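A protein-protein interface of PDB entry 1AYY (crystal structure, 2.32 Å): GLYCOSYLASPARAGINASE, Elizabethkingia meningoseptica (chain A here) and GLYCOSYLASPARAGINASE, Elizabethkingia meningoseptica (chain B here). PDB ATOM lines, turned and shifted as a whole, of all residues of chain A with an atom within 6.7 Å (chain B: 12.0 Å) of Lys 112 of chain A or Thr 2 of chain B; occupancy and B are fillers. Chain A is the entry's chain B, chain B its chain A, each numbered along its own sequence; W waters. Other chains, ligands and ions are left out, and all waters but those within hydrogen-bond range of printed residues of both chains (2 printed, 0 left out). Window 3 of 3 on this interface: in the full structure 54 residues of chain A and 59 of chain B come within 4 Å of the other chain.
Of chain B, only Thr 2 (3.0 Å) and Asn 3 (2.8 Å) come within 4 Å of Lys 112 of chain A. Thr 2 of chain B touches just one residue of chain A: Lys 112. No residue of chain B comes within 4 Å of Asn 110 of chain A. Printed residues of chain A within 4 Å of Pro 5 of chain B: Leu 7 and Gln 131. Of the printed residues of chain A, Ile 6 of chain B touches Leu 7 (2.9 Å), Leu 109 (3.7 Å) and Gly 113 (3.8 Å). Printed residues of chain B within 4 Å of Leu 109 of chain A: Ile 6 (3.7 Å). Of the printed residues of chain A, Asn 3 of chain B touches Lys 112 (2.8 Å) and Gly 113 (3.4 Å). The nearest residue of chain B that does not touch Lys 112 of chain A is Lys 4 of chain B (5.4 Å). The nearest residue of chain A that does not touch Thr 2 of chain B is Lys 111 of chain A (4.4 Å).
The side-chain amide oxygen (OD1) of Asn 110 of chain A is in hydrogen-bond range of the backbone NH (N) of Lys 112 of chain A (3.1 Å). The side-chain amide oxygen of Asn 110 of chain A lies within hydrogen-bond range of the backbone NH of Gly 113 of chain A, at 3.2 Å.
Water W2 lies within hydrogen-bond range of the side-chain amide oxygen (OD1) of Asn 3 of chain B (2.5 Å), the backbone carbonyl oxygen (O) of Pro 5 of chain B (3.0 Å) and the backbone NH (N) of Gln 131 of chain A (3.1 Å). Water W1 lies within hydrogen-bond range of O of Gly 113 of chain A (2.8 Å) and ND2 of Asn 3 of chain B (3.0 Å).
Of the 8 printed residues of chain B, 6 touch a printed residue of chain A. Hydrophobic or aromatic side chains of chain B that line the printed part of chain A: Pro 5, Ile 6 and Trp 22. Of the 9 printed residues of chain A, 5 touch a printed residue of chain B. Hydrophobic or aromatic side chains of chain A that line the printed part of chain B: Leu 7 and Leu 109. Along chain A the printed residues that touch a printed residue of chain B span positions 7 to 131. Among the printed residues, no Asp or Glu carboxylate lies within 4 Å of a Lys or Arg side-chain nitrogen of the other chain.
The backbone NH of Asn 3 of chain B sits at hydrogen-bond distance from the backbone carbonyl oxygen of Lys 112 of chain A (2.8 Å). The backbone carbonyl oxygen (O) of Lys 4 of chain B sits close to the side-chain amide oxygen (OE1) of Gln 131 of chain A (3.1 Å). The backbone carbonyl oxygen of Ile 6 of chain B lies within hydrogen-bond range of the backbone NH of Leu 7 of chain A, 2.9 Å away.
Leu 7 of chain A touches Lys 4 of chain B. Pro 5 of chain B touches Leu 7 of chain A. Ile 6 of chain B touches Leu 109 of chain A. Lys 112 of chain A touches Thr 2 of chain B (O to CA, 3.0 Å). Gly 113 of chain A touches Asn 3 of chain B (CA to O, 3.4 Å). Gly 113 of chain A touches Ile 6 of chain B. Pro 5 of chain B touches Gln 131 of chain A (CD to OE1, 3.9 Å). N of Gln 131 of chain A touches CH2 of Trp 22 of chain B (3.7 Å).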
ATOM      1  N   LEU A   7     -31.027   1.867 -15.664  1.00  0.00           N
ATOM      2  CA  LEU A   7     -31.115   1.274 -16.993  1.00  0.00           C
ATOM      3  C   LEU A   7     -32.583   0.897 -17.181  1.00  0.00           C
ATOM      4  O   LEU A   7     -33.106   0.042 -16.463  1.00  0.00           O
ATOM      5  CB  LEU A   7     -30.233   0.024 -17.074  1.00  0.00           C
ATOM      6  CG  LEU A   7     -30.289  -0.834 -18.340  1.00  0.00           C
ATOM      7  CD1 LEU A   7     -29.560  -0.140 -19.483  1.00  0.00           C
ATOM      8  CD2 LEU A   7     -29.654  -2.187 -18.057  1.00  0.00           C
ATOM      9  N   ILE A  46     -21.359   1.720 -22.698  1.00  0.00           N
ATOM     10  CA  ILE A  46     -20.626   1.014 -21.646  1.00  0.00           C
ATOM     11  C   ILE A  46     -21.370   0.905 -20.316  1.00  0.00           C
ATOM     12  O   ILE A  46     -21.622  -0.196 -19.823  1.00  0.00           O
ATOM     13  CB  ILE A  46     -19.268   1.695 -21.380  1.00  0.00           C
ATOM     14  CG1 ILE A  46     -18.567   1.986 -22.709  1.00  0.00           C
ATOM     15  CG2 ILE A  46     -18.400   0.805 -20.508  1.00  0.00           C
ATOM     16  CD1 ILE A  46     -17.809   3.295 -22.729  1.00  0.00           C
ATOM     17  N   LEU A 109     -22.982   0.749 -12.895  1.00  0.00           N
ATOM     18  CA  LEU A 109     -23.874  -0.159 -13.598  1.00  0.00           C
ATOM     19  C   LEU A 109     -23.497  -0.199 -15.077  1.00  0.00           C
ATOM     20  O   LEU A 109     -23.135   0.822 -15.657  1.00  0.00           O
ATOM     21  CB  LEU A 109     -25.317   0.325 -13.429  1.00  0.00           C
ATOM     22  CG  LEU A 109     -26.456  -0.482 -14.052  1.00  0.00           C
ATOM     23  CD1 LEU A 109     -26.838  -1.637 -13.136  1.00  0.00           C
ATOM     24  CD2 LEU A 109     -27.649   0.436 -14.279  1.00  0.00           C
ATOM     25  N   ASN A 110     -23.570  -1.378 -15.686  1.00  0.00           N
ATOM     26  CA  ASN A 110     -23.240  -1.508 -17.101  1.00  0.00           C
ATOM     27  C   ASN A 110     -24.479  -1.795 -17.945  1.00  0.00           C
ATOM     28  O   ASN A 110     -25.600  -1.824 -17.430  1.00  0.00           O
ATOM     29  CB  ASN A 110     -22.183  -2.601 -17.312  1.00  0.00           C
ATOM     30  CG  ASN A 110     -22.645  -3.967 -16.845  1.00  0.00           C
ATOM     31  OD1 ASN A 110     -23.836  -4.203 -16.647  1.00  0.00           O
ATOM     32  ND2 ASN A 110     -21.697  -4.878 -16.667  1.00  0.00           N
ATOM     33  N   LYS A 111     -24.271  -2.008 -19.240  1.00  0.00           N
ATOM     34  CA  LYS A 111     -25.364  -2.271 -20.173  1.00  0.00           C
ATOM     35  C   LYS A 111     -26.109  -3.583 -19.942  1.00  0.00           C
ATOM     36  O   LYS A 111     -27.272  -3.712 -20.324  1.00  0.00           O
ATOM     37  CB  LYS A 111     -24.837  -2.232 -21.609  1.00  0.00           C
ATOM     38  CG  LYS A 111     -24.771  -0.834 -22.205  1.00  0.00           C
ATOM     39  CD  LYS A 111     -26.121  -0.131 -22.122  1.00  0.00           C
ATOM     40  CE  LYS A 111     -27.046  -0.572 -23.247  1.00  0.00           C
ATOM     41  NZ  LYS A 111     -27.414   0.553 -24.150  1.00  0.00           N
ATOM     42  N   LYS A 112     -25.445  -4.554 -19.323  1.00  0.00           N
ATOM     43  CA  LYS A 112     -26.069  -5.846 -19.061  1.00  0.00           C
ATOM     44  C   LYS A 112     -26.883  -5.828 -17.772  1.00  0.00           C
ATOM     45  O   LYS A 112     -27.458  -6.844 -17.377  1.00  0.00           O
ATOM     46  CB  LYS A 112     -25.004  -6.941 -18.974  1.00  0.00           C
ATOM     47  CG  LYS A 112     -24.141  -7.062 -20.220  1.00  0.00           C
ATOM     48  CD  LYS A 112     -23.740  -8.505 -20.479  1.00  0.00           C
ATOM     49  CE  LYS A 112     -23.691  -8.807 -21.969  1.00  0.00           C
ATOM     50  NZ  LYS A 112     -23.812 -10.266 -22.242  1.00  0.00           N
ATOM     51  N   GLY A 113     -26.930  -4.670 -17.121  1.00  0.00           N
ATOM     52  CA  GLY A 113     -27.676  -4.556 -15.883  1.00  0.00           C
ATOM     53  C   GLY A 113     -26.850  -4.969 -14.681  1.00  0.00           C
ATOM     54  O   GLY A 113     -27.360  -5.052 -13.563  1.00  0.00           O
ATOM     55  N   GLU A 114     -25.570  -5.242 -14.912  1.00  0.00           N
ATOM     56  CA  GLU A 114     -24.666  -5.633 -13.839  1.00  0.00           C
ATOM     57  C   GLU A 114     -24.315  -4.384 -13.041  1.00  0.00           C
ATOM     58  O   GLU A 114     -24.114  -3.311 -13.610  1.00  0.00           O
ATOM     59  CB  GLU A 114     -23.387  -6.249 -14.412  1.00  0.00           C
ATOM     60  CG  GLU A 114     -23.525  -7.696 -14.855  1.00  0.00           C
ATOM     61  CD  GLU A 114     -22.379  -8.139 -15.748  1.00  0.00           C
ATOM     62  OE1 GLU A 114     -22.363  -7.757 -16.936  1.00  0.00           O
ATOM     63  OE2 GLU A 114     -21.492  -8.868 -15.262  1.00  0.00           O
ATOM     64  N   GLN A 131     -36.166  -6.098 -10.925  1.00  0.00           N
ATOM     65  CA  GLN A 131     -37.371  -6.916 -10.994  1.00  0.00           C
ATOM     66  C   GLN A 131     -37.529  -7.859  -9.806  1.00  0.00           C
ATOM     67  O   GLN A 131     -38.616  -8.383  -9.562  1.00  0.00           O
ATOM     68  CB  GLN A 131     -37.376  -7.716 -12.298  1.00  0.00           C
ATOM     69  CG  GLN A 131     -37.410  -6.846 -13.546  1.00  0.00           C
ATOM     70  CD  GLN A 131     -37.959  -7.575 -14.758  1.00  0.00           C
ATOM     71  OE1 GLN A 131     -37.576  -7.289 -15.893  1.00  0.00           O
ATOM     72  NE2 GLN A 131     -38.862  -8.522 -14.524  1.00  0.00           N
ATOM     73  N   THR B   2     -29.823  -9.808 -19.420  1.00  0.00           N
ATOM     74  CA  THR B   2     -29.556  -8.516 -18.797  1.00  0.00           C
ATOM     75  C   THR B   2     -30.545  -8.233 -17.672  1.00  0.00           C
ATOM     76  O   THR B   2     -31.694  -8.673 -17.715  1.00  0.00           O
ATOM     77  CB  THR B   2     -29.643  -7.367 -19.822  1.00  0.00           C
ATOM     78  OG1 THR B   2     -31.017  -7.096 -20.121  1.00  0.00           O
ATOM     79  CG2 THR B   2     -28.914  -7.736 -21.103  1.00  0.00           C
ATOM     80  N   ASN B   3     -30.089  -7.491 -16.668  1.00  0.00           N
ATOM     81  CA  ASN B   3     -30.919  -7.149 -15.524  1.00  0.00           C
ATOM     82  C   ASN B   3     -31.516  -5.757 -15.687  1.00  0.00           C
ATOM     83  O   ASN B   3     -31.006  -4.789 -15.130  1.00  0.00           O
ATOM     84  CB  ASN B   3     -30.091  -7.210 -14.236  1.00  0.00           C
ATOM     85  CG  ASN B   3     -30.950  -7.368 -13.006  1.00  0.00           C
ATOM     86  OD1 ASN B   3     -32.169  -7.235 -13.076  1.00  0.00           O
ATOM     87  ND2 ASN B   3     -30.322  -7.650 -11.865  1.00  0.00           N
ATOM     88  N   LYS B   4     -32.598  -5.660 -16.449  1.00  0.00           N
ATOM     89  CA  LYS B   4     -33.249  -4.379 -16.679  1.00  0.00           C
ATOM     90  C   LYS B   4     -34.764  -4.523 -16.614  1.00  0.00           C
ATOM     91  O   LYS B   4     -35.314  -5.551 -17.012  1.00  0.00           O
ATOM     92  CB  LYS B   4     -32.843  -3.817 -18.043  1.00  0.00           C
ATOM     93  CG  LYS B   4     -33.493  -4.518 -19.222  1.00  0.00           C
ATOM     94  CD  LYS B   4     -33.275  -3.740 -20.500  1.00  0.00           C
ATOM     95  CE  LYS B   4     -33.490  -4.621 -21.716  1.00  0.00           C
ATOM     96  NZ  LYS B   4     -34.938  -4.756 -22.044  1.00  0.00           N
ATOM     97  N   PRO B   5     -35.458  -3.489 -16.106  1.00  0.00           N
ATOM     98  CA  PRO B   5     -34.866  -2.240 -15.614  1.00  0.00           C
ATOM     99  C   PRO B   5     -34.269  -2.372 -14.213  1.00  0.00           C
ATOM    100  O   PRO B   5     -34.645  -3.259 -13.443  1.00  0.00           O
ATOM    101  CB  PRO B   5     -36.030  -1.257 -15.649  1.00  0.00           C
ATOM    102  CG  PRO B   5     -37.233  -2.110 -15.422  1.00  0.00           C
ATOM    103  CD  PRO B   5     -36.927  -3.483 -15.982  1.00  0.00           C
ATOM    104  N   ILE B   6     -33.335  -1.481 -13.892  1.00  0.00           N
ATOM    105  CA  ILE B   6     -32.678  -1.487 -12.588  1.00  0.00           C
ATOM    106  C   ILE B   6     -32.174  -0.085 -12.240  1.00  0.00           C
ATOM    107  O   ILE B   6     -31.685   0.641 -13.108  1.00  0.00           O
ATOM    108  CB  ILE B   6     -31.490  -2.477 -12.576  1.00  0.00           C
ATOM    109  CG1 ILE B   6     -30.836  -2.497 -11.194  1.00  0.00           C
ATOM    110  CG2 ILE B   6     -30.478  -2.092 -13.645  1.00  0.00           C
ATOM    111  CD1 ILE B   6     -29.763  -3.560 -11.042  1.00  0.00           C
ATOM    112  N   VAL B   7     -32.306   0.296 -10.973  1.00  0.00           N
ATOM    113  CA  VAL B   7     -31.863   1.613 -10.530  1.00  0.00           C
ATOM    114  C   VAL B   7     -30.980   1.523  -9.282  1.00  0.00           C
ATOM    115  O   VAL B   7     -31.182   0.663  -8.421  1.00  0.00           O
ATOM    116  CB  VAL B   7     -33.082   2.541 -10.254  1.00  0.00           C
ATOM    117  CG1 VAL B   7     -34.141   1.796  -9.455  1.00  0.00           C
ATOM    118  CG2 VAL B   7     -32.637   3.796  -9.517  1.00  0.00           C
ATOM    119  N   LEU B   8     -29.995   2.415  -9.198  1.00  0.00           N
ATOM    120  CA  LEU B   8     -29.066   2.452  -8.073  1.00  0.00           C
ATOM    121  C   LEU B   8     -28.935   3.874  -7.532  1.00  0.00           C
ATOM    122  O   LEU B   8     -28.795   4.822  -8.303  1.00  0.00           O
ATOM    123  CB  LEU B   8     -27.681   1.967  -8.518  1.00  0.00           C
ATOM    124  CG  LEU B   8     -27.321   0.485  -8.415  1.00  0.00           C
ATOM    125  CD1 LEU B   8     -25.816   0.321  -8.577  1.00  0.00           C
ATOM    126  CD2 LEU B   8     -27.767  -0.065  -7.078  1.00  0.00           C
ATOM    127  N   TRP B  22     -38.492   3.817  -9.760  1.00  0.00           N
ATOM    128  CA  TRP B  22     -39.059   2.565 -10.239  1.00  0.00           C
ATOM    129  C   TRP B  22     -40.444   2.775 -10.838  1.00  0.00           C
ATOM    130  O   TRP B  22     -40.808   2.125 -11.818  1.00  0.00           O
ATOM    131  CB  TRP B  22     -39.150   1.558  -9.091  1.00  0.00           C
ATOM    132  CG  TRP B  22     -39.493   0.174  -9.543  1.00  0.00           C
ATOM    133  CD1 TRP B  22     -40.643  -0.515  -9.281  1.00  0.00           C
ATOM    134  CD2 TRP B  22     -38.672  -0.699 -10.330  1.00  0.00           C
ATOM    135  NE1 TRP B  22     -40.588  -1.764  -9.855  1.00  0.00           N
ATOM    136  CE2 TRP B  22     -39.389  -1.902 -10.504  1.00  0.00           C
ATOM    137  CE3 TRP B  22     -37.399  -0.579 -10.905  1.00  0.00           C
ATOM    138  CZ2 TRP B  22     -38.875  -2.981 -11.229  1.00  0.00           C
ATOM    139  CZ3 TRP B  22     -36.888  -1.654 -11.625  1.00  0.00           C
ATOM    140  CH2 TRP B  22     -37.626  -2.838 -11.779  1.00  0.00           C
HETATM  141  O   HOH W   1     -27.312  -7.331 -11.894  1.00  0.00           O
HETATM  142  O   HOH W   2     -34.489  -6.272 -13.515  1.00  0.00           O
